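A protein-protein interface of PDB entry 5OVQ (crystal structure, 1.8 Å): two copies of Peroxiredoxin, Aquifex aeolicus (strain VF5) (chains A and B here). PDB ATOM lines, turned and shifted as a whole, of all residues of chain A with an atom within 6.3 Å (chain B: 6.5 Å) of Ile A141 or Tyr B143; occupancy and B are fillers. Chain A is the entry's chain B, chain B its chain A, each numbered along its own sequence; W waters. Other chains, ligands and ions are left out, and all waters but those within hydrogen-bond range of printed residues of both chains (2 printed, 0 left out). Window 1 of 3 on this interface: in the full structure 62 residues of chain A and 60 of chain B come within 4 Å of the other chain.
The side-chain carboxylate of Glu B153 lies within hydrogen-bond range of the side-chain hydroxyl of Tyr A143, 2.6 Å away. The guanidinium group (NH2) of Arg A156 sits at hydrogen-bond distance from the backbone carbonyl oxygen (O) of Gly B148 (3.1 Å). N of Tyr B142 lies within hydrogen-bond range of O of Met A140. O of Met B140 lies within hydrogen-bond range of N of Tyr A142 (2.8 Å). ND2 of Asn B150 lies within hydrogen-bond range of OE2 of Glu A153, at 2.7 Å. The side-chain carboxylate of Glu A153 sits at hydrogen-bond distance from the side-chain hydroxyl of Tyr B143.
O of Arg B126 lies close to NH1 of Arg B149 (3.4 Å). N of Tyr A143 sits at hydrogen-bond distance from O of Arg A126 (2.9 Å). OE2 of Glu A153 is in salt-bridge range of NE of Arg A156, at 2.7 Å. The backbone carbonyl oxygen (O) of Pro B144 sits close to the guanidinium group (NE) of Arg B126 (3.2 Å). The side-chain amide oxygen (OD1) of Asn B150 sits at hydrogen-bond distance from the backbone NH (N) of Glu B153 (3.1 Å). NE of Arg B149 is in salt-bridge range of OE1 of Glu B52, at 2.8 Å.
Leu A9 touches Gln B119 (CB to CG, 3.8 Å). Arg A138 touches Pro B144. Tyr B142 touches Ala A139 (O to CA, 3.5 Å). Pro B144 touches Ala A139. Ile A141 touches Met B140 (C to O, 3.7 Å). CG1 of Ile A141 touches CG2 of Ile B141, 3.6 Å away. OH of Tyr B143 touches CD1 of Ile A141 (3.8 Å). Tyr B143 touches Arg A156 (CE1 to NH2, 3.9 Å). Arg A156 touches Arg B149 (NH2 to C, 3.8 Å). Arg A156 touches Asn B150 (NH2 to N, 3.8 Å).
Of the printed residues of chain B, Tyr A143 touches Glu B153. Glu B52 touches none of the printed residues of chain A. Of the printed residues of chain A, Gln B119 touches Leu A9 (3.8 Å). Leu B128 touches none of the printed residues of chain A. Printed residues of chain A within 4 Å of Tyr B143: Ile A141, Glu A153, Arg A156 and Leu A157. The nearest printed residue of chain A that does not touch Tyr B143 is Leu A9 (4.3 Å).
Of the 16 printed residues of chain A, 10 touch a printed residue of chain B. Hydrophobic or aromatic side chains of chain A within 4 Å of the printed part of chain B: Leu A9, Ala A139, Met A140, Ile A141, Tyr A142, Tyr A143 and Leu A157.
Met A140 touches Ile B141, and with the chains exchanged Ile A141 touches Met B140. Met A140 touches Tyr B142, and with the chains exchanged Tyr A142 touches Met B140. Ile A141 touches its own counterpart, Ile B141. Ile A141 touches Tyr B143, but with the chains exchanged Tyr A143 does not touch Ile B141 (4.1 Å). Positions printed for both chains: 126, 127, 128, 140, 141, 142, 143, 149 and 153. Of the 19 pairs that touch across the chains among the printed residues, 7 have their exchanged pair printed and touching as well.
Water W2 lies within hydrogen-bond range of the side-chain hydroxyl (OG1) of Thr B146 and the guanidinium group (NH2) of Arg A138. Water W1 lies within hydrogen-bond range of the backbone carbonyl oxygen of Gly B148 and the guanidinium group of Arg A156.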
ATOM      1  N   LEU A   9      -7.085  12.302   0.821  1.00  0.00           N
ATOM      2  CA  LEU A   9      -6.131  12.786  -0.126  1.00  0.00           C
ATOM      3  C   LEU A   9      -5.260  11.652  -0.625  1.00  0.00           C
ATOM      4  O   LEU A   9      -4.874  10.846   0.114  1.00  0.00           O
ATOM      5  CB  LEU A   9      -5.261  13.870   0.465  1.00  0.00           C
ATOM      6  CG  LEU A   9      -5.981  15.127   0.892  1.00  0.00           C
ATOM      7  CD1 LEU A   9      -5.016  16.108   1.497  1.00  0.00           C
ATOM      8  CD2 LEU A   9      -6.689  15.747  -0.268  1.00  0.00           C
ATOM      9  N   ARG A 126     -19.374  25.505   1.095  1.00  0.00           N
ATOM     10  CA  ARG A 126     -18.583  25.868  -0.083  1.00  0.00           C
ATOM     11  C   ARG A 126     -17.329  24.999  -0.139  1.00  0.00           C
ATOM     12  O   ARG A 126     -16.214  25.446   0.120  1.00  0.00           O
ATOM     13  CB  ARG A 126     -18.207  27.340  -0.041  1.00  0.00           C
ATOM     14  CG  ARG A 126     -19.366  28.252   0.126  1.00  0.00           C
ATOM     15  CD  ARG A 126     -18.931  29.726   0.059  1.00  0.00           C
ATOM     16  NE  ARG A 126     -20.137  30.457   0.345  1.00  0.00           N
ATOM     17  CZ  ARG A 126     -21.070  30.657  -0.563  1.00  0.00           C
ATOM     18  NH1 ARG A 126     -20.845  30.257  -1.810  1.00  0.00           N
ATOM     19  NH2 ARG A 126     -22.203  31.241  -0.223  1.00  0.00           N
ATOM     20  N   ALA A 127     -17.534  23.748  -0.516  1.00  0.00           N
ATOM     21  CA  ALA A 127     -16.446  22.791  -0.603  1.00  0.00           C
ATOM     22  C   ALA A 127     -15.846  22.803  -1.999  1.00  0.00           C
ATOM     23  O   ALA A 127     -16.532  23.044  -2.994  1.00  0.00           O
ATOM     24  CB  ALA A 127     -16.940  21.386  -0.246  1.00  0.00           C
ATOM     25  N   LEU A 128     -14.546  22.551  -2.072  1.00  0.00           N
ATOM     26  CA  LEU A 128     -13.900  22.484  -3.371  1.00  0.00           C
ATOM     27  C   LEU A 128     -12.811  21.429  -3.333  1.00  0.00           C
ATOM     28  O   LEU A 128     -12.073  21.335  -2.356  1.00  0.00           O
ATOM     29  CB  LEU A 128     -13.326  23.860  -3.757  1.00  0.00           C
ATOM     30  CG  LEU A 128     -12.692  23.950  -5.135  1.00  0.00           C
ATOM     31  CD1 LEU A 128     -12.909  25.351  -5.728  1.00  0.00           C
ATOM     32  CD2 LEU A 128     -11.174  23.611  -5.078  1.00  0.00           C
ATOM     33  N   PHE A 129     -12.700  20.662  -4.419  1.00  0.00           N
ATOM     34  CA  PHE A 129     -11.837  19.495  -4.481  1.00  0.00           C
ATOM     35  C   PHE A 129     -11.057  19.550  -5.773  1.00  0.00           C
ATOM     36  O   PHE A 129     -11.653  19.696  -6.844  1.00  0.00           O
ATOM     37  CB  PHE A 129     -12.673  18.206  -4.431  1.00  0.00           C
ATOM     38  CG  PHE A 129     -13.536  18.119  -3.225  1.00  0.00           C
ATOM     39  CD1 PHE A 129     -13.014  17.687  -2.018  1.00  0.00           C
ATOM     40  CD2 PHE A 129     -14.848  18.577  -3.267  1.00  0.00           C
ATOM     41  CE1 PHE A 129     -13.791  17.643  -0.888  1.00  0.00           C
ATOM     42  CE2 PHE A 129     -15.637  18.554  -2.132  1.00  0.00           C
ATOM     43  CZ  PHE A 129     -15.113  18.082  -0.939  1.00  0.00           C
ATOM     44  N   ARG A 138      -6.518  15.409  -4.748  1.00  0.00           N
ATOM     45  CA  ARG A 138      -5.221  16.015  -4.467  1.00  0.00           C
ATOM     46  C   ARG A 138      -5.271  17.091  -3.400  1.00  0.00           C
ATOM     47  O   ARG A 138      -4.303  17.251  -2.657  1.00  0.00           O
ATOM     48  CB  ARG A 138      -4.619  16.599  -5.746  1.00  0.00           C
ATOM     49  CG  ARG A 138      -4.472  15.557  -6.826  1.00  0.00           C
ATOM     50  CD  ARG A 138      -3.479  14.489  -6.425  1.00  0.00           C
ATOM     51  NE  ARG A 138      -2.153  15.091  -6.300  1.00  0.00           N
ATOM     52  CZ  ARG A 138      -1.285  15.197  -7.302  1.00  0.00           C
ATOM     53  NH1 ARG A 138      -1.584  14.720  -8.507  1.00  0.00           N
ATOM     54  NH2 ARG A 138      -0.109  15.784  -7.094  1.00  0.00           N
ATOM     55  N   ALA A 139      -6.385  17.803  -3.268  1.00  0.00           N
ATOM     56  CA  ALA A 139      -6.413  18.904  -2.319  1.00  0.00           C
ATOM     57  C   ALA A 139      -7.865  19.272  -2.115  1.00  0.00           C
ATOM     58  O   ALA A 139      -8.703  19.000  -2.973  1.00  0.00           O
ATOM     59  CB  ALA A 139      -5.606  20.106  -2.838  1.00  0.00           C
ATOM     60  N   MET A 140      -8.165  19.894  -0.980  1.00  0.00           N
ATOM     61  CA  MET A 140      -9.561  20.234  -0.807  1.00  0.00           C
ATOM     62  C   MET A 140      -9.662  21.411   0.142  1.00  0.00           C
ATOM     63  O   MET A 140      -8.787  21.638   0.974  1.00  0.00           O
ATOM     64  CB  MET A 140     -10.356  19.029  -0.292  1.00  0.00           C
ATOM     65  CG  MET A 140     -10.050  18.599   1.127  1.00  0.00           C
ATOM     66  SD  MET A 140     -10.725  16.951   1.371  1.00  0.00           S
ATOM     67  CE  MET A 140      -9.396  16.180   2.280  1.00  0.00           C
ATOM     68  N   ILE A 141     -10.751  22.153  -0.001  1.00  0.00           N
ATOM     69  CA  ILE A 141     -11.027  23.330   0.802  1.00  0.00           C
ATOM     70  C   ILE A 141     -12.486  23.288   1.232  1.00  0.00           C
ATOM     71  O   ILE A 141     -13.346  22.781   0.509  1.00  0.00           O
ATOM     72  CB  ILE A 141     -10.714  24.588  -0.030  1.00  0.00           C
ATOM     73  CG1 ILE A 141      -9.200  24.769  -0.128  1.00  0.00           C
ATOM     74  CG2 ILE A 141     -11.441  25.812   0.491  1.00  0.00           C
ATOM     75  CD1 ILE A 141      -8.812  25.839  -1.102  1.00  0.00           C
ATOM     76  N   TYR A 142     -12.762  23.783   2.435  1.00  0.00           N
ATOM     77  CA  TYR A 142     -14.135  23.884   2.924  1.00  0.00           C
ATOM     78  C   TYR A 142     -14.342  25.279   3.483  1.00  0.00           C
ATOM     79  O   TYR A 142     -13.956  25.554   4.623  1.00  0.00           O
ATOM     80  CB  TYR A 142     -14.453  22.830   4.002  1.00  0.00           C
ATOM     81  CG  TYR A 142     -14.434  21.387   3.558  1.00  0.00           C
ATOM     82  CD1 TYR A 142     -13.240  20.673   3.460  1.00  0.00           C
ATOM     83  CD2 TYR A 142     -15.621  20.737   3.219  1.00  0.00           C
ATOM     84  CE1 TYR A 142     -13.228  19.358   3.043  1.00  0.00           C
ATOM     85  CE2 TYR A 142     -15.619  19.423   2.796  1.00  0.00           C
ATOM     86  CZ  TYR A 142     -14.417  18.726   2.737  1.00  0.00           C
ATOM     87  OH  TYR A 142     -14.389  17.414   2.329  1.00  0.00           O
ATOM     88  N   TYR A 143     -15.021  26.175   2.670  1.00  0.00           N
ATOM     89  CA  TYR A 143     -15.374  27.484   3.193  1.00  0.00           C
ATOM     90  C   TYR A 143     -16.834  27.504   3.643  1.00  0.00           C
ATOM     91  O   TYR A 143     -17.657  26.707   3.170  1.00  0.00           O
ATOM     92  CB  TYR A 143     -15.144  28.579   2.137  1.00  0.00           C
ATOM     93  CG  TYR A 143     -13.708  29.078   2.033  1.00  0.00           C
ATOM     94  CD1 TYR A 143     -13.425  30.280   1.401  1.00  0.00           C
ATOM     95  CD2 TYR A 143     -12.649  28.350   2.553  1.00  0.00           C
ATOM     96  CE1 TYR A 143     -12.131  30.750   1.289  1.00  0.00           C
ATOM     97  CE2 TYR A 143     -11.337  28.814   2.446  1.00  0.00           C
ATOM     98  CZ  TYR A 143     -11.088  30.010   1.813  1.00  0.00           C
ATOM     99  OH  TYR A 143      -9.786  30.474   1.702  1.00  0.00           O
ATOM    100  N   ARG A 149     -15.125  32.117  -2.224  1.00  0.00           N
ATOM    101  CA  ARG A 149     -13.799  31.562  -2.421  1.00  0.00           C
ATOM    102  C   ARG A 149     -12.928  32.498  -3.266  1.00  0.00           C
ATOM    103  O   ARG A 149     -13.373  33.530  -3.781  1.00  0.00           O
ATOM    104  CB  ARG A 149     -13.916  30.168  -3.039  1.00  0.00           C
ATOM    105  CG  ARG A 149     -14.439  29.119  -2.023  1.00  0.00           C
ATOM    106  CD  ARG A 149     -15.035  27.860  -2.675  1.00  0.00           C
ATOM    107  NE  ARG A 149     -16.386  28.154  -3.168  1.00  0.00           N
ATOM    108  CZ  ARG A 149     -17.325  27.241  -3.386  1.00  0.00           C
ATOM    109  NH1 ARG A 149     -17.073  25.960  -3.153  1.00  0.00           N
ATOM    110  NH2 ARG A 149     -18.525  27.617  -3.811  1.00  0.00           N
ATOM    111  N   GLU A 153      -6.607  31.567  -6.321  1.00  0.00           N
ATOM    112  CA  GLU A 153      -5.902  30.573  -5.509  1.00  0.00           C
ATOM    113  C   GLU A 153      -6.227  29.157  -5.967  1.00  0.00           C
ATOM    114  O   GLU A 153      -5.383  28.255  -5.849  1.00  0.00           O
ATOM    115  CB  GLU A 153      -6.215  30.778  -4.021  1.00  0.00           C
ATOM    116  CG  GLU A 153      -5.696  29.643  -3.095  1.00  0.00           C
ATOM    117  CD  GLU A 153      -4.184  29.441  -3.191  1.00  0.00           C
ATOM    118  OE1 GLU A 153      -3.707  28.368  -2.760  1.00  0.00           O
ATOM    119  OE2 GLU A 153      -3.479  30.343  -3.706  1.00  0.00           O
ATOM    120  N   VAL A 154      -7.435  28.932  -6.493  1.00  0.00           N
ATOM    121  CA  VAL A 154      -7.731  27.633  -7.088  1.00  0.00           C
ATOM    122  C   VAL A 154      -6.849  27.394  -8.295  1.00  0.00           C
ATOM    123  O   VAL A 154      -6.297  26.306  -8.476  1.00  0.00           O
ATOM    124  CB  VAL A 154      -9.222  27.527  -7.460  1.00  0.00           C
ATOM    125  CG1 VAL A 154      -9.487  26.198  -8.132  1.00  0.00           C
ATOM    126  CG2 VAL A 154     -10.072  27.693  -6.219  1.00  0.00           C
ATOM    127  N   ARG A 156      -3.932  28.784  -8.860  1.00  0.00           N
ATOM    128  CA  ARG A 156      -2.564  28.630  -8.362  1.00  0.00           C
ATOM    129  C   ARG A 156      -2.358  27.230  -7.815  1.00  0.00           C
ATOM    130  O   ARG A 156      -1.316  26.612  -8.033  1.00  0.00           O
ATOM    131  CB  ARG A 156      -2.279  29.667  -7.271  1.00  0.00           C
ATOM    132  CG  ARG A 156      -0.786  29.756  -6.875  1.00  0.00           C
ATOM    133  CD  ARG A 156      -0.589  30.479  -5.540  1.00  0.00           C
ATOM    134  NE  ARG A 156      -0.993  29.624  -4.436  1.00  0.00           N
ATOM    135  CZ  ARG A 156      -0.219  28.704  -3.852  1.00  0.00           C
ATOM    136  NH1 ARG A 156       1.043  28.507  -4.250  1.00  0.00           N
ATOM    137  NH2 ARG A 156      -0.726  27.979  -2.862  1.00  0.00           N
ATOM    138  N   LEU A 157      -3.363  26.712  -7.109  1.00  0.00           N
ATOM    139  CA  LEU A 157      -3.275  25.365  -6.559  1.00  0.00           C
ATOM    140  C   LEU A 157      -3.105  24.335  -7.666  1.00  0.00           C
ATOM    141  O   LEU A 157      -2.260  23.437  -7.579  1.00  0.00           O
ATOM    142  CB  LEU A 157      -4.530  25.096  -5.745  1.00  0.00           C
ATOM    143  CG  LEU A 157      -4.707  23.697  -5.176  1.00  0.00           C
ATOM    144  CD1 LEU A 157      -3.476  23.302  -4.316  1.00  0.00           C
ATOM    145  CD2 LEU A 157      -5.947  23.704  -4.339  1.00  0.00           C
ATOM    146  N   GLU B  52       6.812  28.068   4.538  1.00  0.00           N
ATOM    147  CA  GLU B  52       5.543  28.504   5.113  1.00  0.00           C
ATOM    148  C   GLU B  52       5.747  29.153   6.470  1.00  0.00           C
ATOM    149  O   GLU B  52       5.108  30.163   6.772  1.00  0.00           O
ATOM    150  CB  GLU B  52       4.587  27.314   5.238  1.00  0.00           C
ATOM    151  CG  GLU B  52       4.127  26.760   3.895  1.00  0.00           C
ATOM    152  CD  GLU B  52       3.247  25.542   4.051  1.00  0.00           C
ATOM    153  OE1 GLU B  52       2.231  25.439   3.335  1.00  0.00           O
ATOM    154  OE2 GLU B  52       3.562  24.710   4.920  1.00  0.00           O
ATOM    155  N   GLN B 119      -1.188   9.801   1.629  1.00  0.00           N
ATOM    156  CA  GLN B 119      -0.160  10.832   1.678  1.00  0.00           C
ATOM    157  C   GLN B 119       0.987  10.394   2.579  1.00  0.00           C
ATOM    158  O   GLN B 119       2.151  10.365   2.162  1.00  0.00           O
ATOM    159  CB  GLN B 119      -0.774  12.132   2.190  1.00  0.00           C
ATOM    160  CG  GLN B 119      -1.634  12.832   1.153  1.00  0.00           C
ATOM    161  CD  GLN B 119      -0.804  13.783   0.318  1.00  0.00           C
ATOM    162  OE1 GLN B 119      -0.433  14.853   0.788  1.00  0.00           O
ATOM    163  NE2 GLN B 119      -0.463  13.377  -0.899  1.00  0.00           N
ATOM    164  N   VAL B 125      -0.872  16.080   6.814  1.00  0.00           N
ATOM    165  CA  VAL B 125      -0.885  16.857   5.578  1.00  0.00           C
ATOM    166  C   VAL B 125      -0.792  18.327   5.958  1.00  0.00           C
ATOM    167  O   VAL B 125      -0.578  18.671   7.130  1.00  0.00           O
ATOM    168  CB  VAL B 125      -2.142  16.565   4.728  1.00  0.00           C
ATOM    169  CG1 VAL B 125      -2.210  15.082   4.328  1.00  0.00           C
ATOM    170  CG2 VAL B 125      -3.414  16.962   5.472  1.00  0.00           C
ATOM    171  N   ARG B 126      -0.961  19.206   4.971  1.00  0.00           N
ATOM    172  CA  ARG B 126      -0.934  20.653   5.198  1.00  0.00           C
ATOM    173  C   ARG B 126      -2.349  21.155   5.457  1.00  0.00           C
ATOM    174  O   ARG B 126      -2.973  21.811   4.621  1.00  0.00           O
ATOM    175  CB  ARG B 126      -0.329  21.370   4.006  1.00  0.00           C
ATOM    176  CG  ARG B 126       1.041  20.887   3.637  1.00  0.00           C
ATOM    177  CD  ARG B 126       1.680  21.736   2.508  1.00  0.00           C
ATOM    178  NE  ARG B 126       2.938  21.071   2.267  1.00  0.00           N
ATOM    179  CZ  ARG B 126       3.989  21.240   3.051  1.00  0.00           C
ATOM    180  NH1 ARG B 126       3.927  22.124   4.040  1.00  0.00           N
ATOM    181  NH2 ARG B 126       5.079  20.528   2.847  1.00  0.00           N
ATOM    182  N   ALA B 127      -2.834  20.856   6.650  1.00  0.00           N
ATOM    183  CA  ALA B 127      -4.173  21.265   7.054  1.00  0.00           C
ATOM    184  C   ALA B 127      -4.124  22.641   7.705  1.00  0.00           C
ATOM    185  O   ALA B 127      -3.128  23.030   8.325  1.00  0.00           O
ATOM    186  CB  ALA B 127      -4.778  20.248   8.026  1.00  0.00           C
ATOM    187  N   LEU B 128      -5.199  23.401   7.526  1.00  0.00           N
ATOM    188  CA  LEU B 128      -5.289  24.691   8.190  1.00  0.00           C
ATOM    189  C   LEU B 128      -6.737  24.955   8.567  1.00  0.00           C
ATOM    190  O   LEU B 128      -7.653  24.642   7.804  1.00  0.00           O
ATOM    191  CB  LEU B 128      -4.725  25.819   7.311  1.00  0.00           C
ATOM    192  CG  LEU B 128      -4.723  27.215   7.930  1.00  0.00           C
ATOM    193  CD1 LEU B 128      -3.520  28.038   7.435  1.00  0.00           C
ATOM    194  CD2 LEU B 128      -6.039  27.971   7.622  1.00  0.00           C
ATOM    195  N   MET B 140     -11.742  25.594   6.659  1.00  0.00           N
ATOM    196  CA  MET B 140     -10.575  24.738   6.726  1.00  0.00           C
ATOM    197  C   MET B 140     -10.119  24.403   5.317  1.00  0.00           C
ATOM    198  O   MET B 140     -10.899  24.468   4.367  1.00  0.00           O
ATOM    199  CB  MET B 140     -10.884  23.456   7.521  1.00  0.00           C
ATOM    200  CG  MET B 140     -11.855  22.490   6.864  1.00  0.00           C
ATOM    201  SD  MET B 140     -12.472  21.282   8.076  1.00  0.00           S
ATOM    202  CE  MET B 140     -14.205  21.227   7.640  1.00  0.00           C
ATOM    203  N   ILE B 141      -8.833  24.088   5.189  1.00  0.00           N
ATOM    204  CA  ILE B 141      -8.242  23.682   3.920  1.00  0.00           C
ATOM    205  C   ILE B 141      -7.301  22.517   4.191  1.00  0.00           C
ATOM    206  O   ILE B 141      -6.721  22.398   5.271  1.00  0.00           O
ATOM    207  CB  ILE B 141      -7.484  24.835   3.209  1.00  0.00           C
ATOM    208  CG1 ILE B 141      -6.167  25.138   3.910  1.00  0.00           C
ATOM    209  CG2 ILE B 141      -8.364  26.102   3.088  1.00  0.00           C
ATOM    210  CD1 ILE B 141      -5.161  25.855   3.033  1.00  0.00           C
ATOM    211  N   TYR B 142      -7.179  21.633   3.210  1.00  0.00           N
ATOM    212  CA  TYR B 142      -6.274  20.492   3.300  1.00  0.00           C
ATOM    213  C   TYR B 142      -5.450  20.471   2.029  1.00  0.00           C
ATOM    214  O   TYR B 142      -5.936  20.038   0.982  1.00  0.00           O
ATOM    215  CB  TYR B 142      -7.038  19.167   3.476  1.00  0.00           C
ATOM    216  CG  TYR B 142      -7.787  18.999   4.766  1.00  0.00           C
ATOM    217  CD1 TYR B 142      -7.237  18.241   5.802  1.00  0.00           C
ATOM    218  CD2 TYR B 142      -9.033  19.582   4.969  1.00  0.00           C
ATOM    219  CE1 TYR B 142      -7.903  18.077   6.998  1.00  0.00           C
ATOM    220  CE2 TYR B 142      -9.694  19.428   6.164  1.00  0.00           C
ATOM    221  CZ  TYR B 142      -9.144  18.662   7.168  1.00  0.00           C
ATOM    222  OH  TYR B 142      -9.822  18.507   8.355  1.00  0.00           O
ATOM    223  N   TYR B 143      -4.167  20.959   2.130  1.00  0.00           N
ATOM    224  CA  TYR B 143      -3.266  20.843   1.006  1.00  0.00           C
ATOM    225  C   TYR B 143      -2.341  19.636   1.188  1.00  0.00           C
ATOM    226  O   TYR B 143      -2.080  19.195   2.308  1.00  0.00           O
ATOM    227  CB  TYR B 143      -2.432  22.138   0.850  1.00  0.00           C
ATOM    228  CG  TYR B 143      -3.135  23.279   0.113  1.00  0.00           C
ATOM    229  CD1 TYR B 143      -2.414  24.380  -0.362  1.00  0.00           C
ATOM    230  CD2 TYR B 143      -4.517  23.277  -0.063  1.00  0.00           C
ATOM    231  CE1 TYR B 143      -3.055  25.440  -1.034  1.00  0.00           C
ATOM    232  CE2 TYR B 143      -5.154  24.317  -0.733  1.00  0.00           C
ATOM    233  CZ  TYR B 143      -4.424  25.401  -1.199  1.00  0.00           C
ATOM    234  OH  TYR B 143      -5.086  26.429  -1.862  1.00  0.00           O
ATOM    235  N   PRO B 144      -1.867  19.053   0.099  1.00  0.00           N
ATOM    236  CA  PRO B 144      -1.038  17.849   0.177  1.00  0.00           C
ATOM    237  C   PRO B 144       0.423  18.174   0.492  1.00  0.00           C
ATOM    238  O   PRO B 144       0.834  19.331   0.554  1.00  0.00           O
ATOM    239  CB  PRO B 144      -1.194  17.263  -1.231  1.00  0.00           C
ATOM    240  CG  PRO B 144      -1.385  18.489  -2.098  1.00  0.00           C
ATOM    241  CD  PRO B 144      -2.227  19.416  -1.283  1.00  0.00           C
ATOM    242  N   LEU B 145       1.218  17.108   0.687  1.00  0.00           N
ATOM    243  CA  LEU B 145       2.610  17.298   1.102  1.00  0.00           C
ATOM    244  C   LEU B 145       3.416  18.119   0.097  1.00  0.00           C
ATOM    245  O   LEU B 145       4.359  18.821   0.485  1.00  0.00           O
ATOM    246  CB  LEU B 145       3.284  15.945   1.306  1.00  0.00           C
ATOM    247  CG  LEU B 145       2.614  14.996   2.297  1.00  0.00           C
ATOM    248  CD1 LEU B 145       3.420  13.711   2.401  1.00  0.00           C
ATOM    249  CD2 LEU B 145       2.473  15.669   3.653  1.00  0.00           C
ATOM    250  N   THR B 146       3.086  18.025  -1.192  1.00  0.00           N
ATOM    251  CA  THR B 146       3.852  18.715  -2.228  1.00  0.00           C
ATOM    252  C   THR B 146       3.709  20.239  -2.216  1.00  0.00           C
ATOM    253  O   THR B 146       4.571  20.930  -2.776  1.00  0.00           O
ATOM    254  CB  THR B 146       3.411  18.246  -3.616  1.00  0.00           C
ATOM    255  OG1 THR B 146       1.977  18.363  -3.727  1.00  0.00           O
ATOM    256  CG2 THR B 146       3.828  16.822  -3.866  1.00  0.00           C
ATOM    257  N   THR B 147       2.643  20.789  -1.637  1.00  0.00           N
ATOM    258  CA  THR B 147       2.099  22.069  -2.106  1.00  0.00           C
ATOM    259  C   THR B 147       1.956  23.080  -0.978  1.00  0.00           C
ATOM    260  O   THR B 147       0.998  23.016  -0.206  1.00  0.00           O
ATOM    261  CB  THR B 147       0.745  21.832  -2.782  1.00  0.00           C
ATOM    262  OG1 THR B 147       0.923  20.899  -3.864  1.00  0.00           O
ATOM    263  CG2 THR B 147       0.188  23.162  -3.357  1.00  0.00           C
ATOM    264  N   GLY B 148       2.848  24.067  -0.941  1.00  0.00           N
ATOM    265  CA  GLY B 148       2.763  25.094   0.082  1.00  0.00           C
ATOM    266  C   GLY B 148       1.511  25.937  -0.059  1.00  0.00           C
ATOM    267  O   GLY B 148       0.956  26.091  -1.141  1.00  0.00           O
ATOM    268  N   ARG B 149       1.087  26.507   1.066  1.00  0.00           N
ATOM    269  CA  ARG B 149      -0.136  27.267   1.168  1.00  0.00           C
ATOM    270  C   ARG B 149       0.079  28.719   0.742  1.00  0.00           C
ATOM    271  O   ARG B 149       1.200  29.178   0.515  1.00  0.00           O
ATOM    272  CB  ARG B 149      -0.668  27.172   2.594  1.00  0.00           C
ATOM    273  CG  ARG B 149      -1.279  25.775   2.870  1.00  0.00           C
ATOM    274  CD  ARG B 149      -1.379  25.412   4.346  1.00  0.00           C
ATOM    275  NE  ARG B 149      -0.083  24.946   4.853  1.00  0.00           N
ATOM    276  CZ  ARG B 149       0.062  24.168   5.921  1.00  0.00           C
ATOM    277  NH1 ARG B 149      -0.999  23.757   6.599  1.00  0.00           N
ATOM    278  NH2 ARG B 149       1.266  23.790   6.299  1.00  0.00           N
ATOM    279  N   ASN B 150      -1.028  29.436   0.635  1.00  0.00           N
ATOM    280  CA  ASN B 150      -1.055  30.840   0.216  1.00  0.00           C
ATOM    281  C   ASN B 150      -1.362  31.662   1.457  1.00  0.00           C
ATOM    282  O   ASN B 150      -2.507  31.714   1.899  1.00  0.00           O
ATOM    283  CB  ASN B 150      -2.103  31.035  -0.872  1.00  0.00           C
ATOM    284  CG  ASN B 150      -2.186  32.475  -1.381  1.00  0.00           C
ATOM    285  OD1 ASN B 150      -1.895  33.425  -0.660  1.00  0.00           O
ATOM    286  ND2 ASN B 150      -2.651  32.631  -2.613  1.00  0.00           N
ATOM    287  N   GLU B 153      -4.064  34.428   1.271  1.00  0.00           N
ATOM    288  CA  GLU B 153      -5.439  33.930   1.261  1.00  0.00           C
ATOM    289  C   GLU B 153      -5.920  33.581   2.664  1.00  0.00           C
ATOM    290  O   GLU B 153      -7.103  33.771   2.976  1.00  0.00           O
ATOM    291  CB  GLU B 153      -5.564  32.732   0.317  1.00  0.00           C
ATOM    292  CG  GLU B 153      -6.941  32.027   0.376  1.00  0.00           C
ATOM    293  CD  GLU B 153      -8.118  32.971   0.081  1.00  0.00           C
ATOM    294  OE1 GLU B 153      -7.893  34.089  -0.430  1.00  0.00           O
ATOM    295  OE2 GLU B 153      -9.284  32.579   0.352  1.00  0.00           O
HETATM  296  O   HOH W   1       2.729  26.118  -3.359  1.00  0.00           O
HETATM  297  O   HOH W   2       0.413  16.234  -4.382  1.00  0.00           O
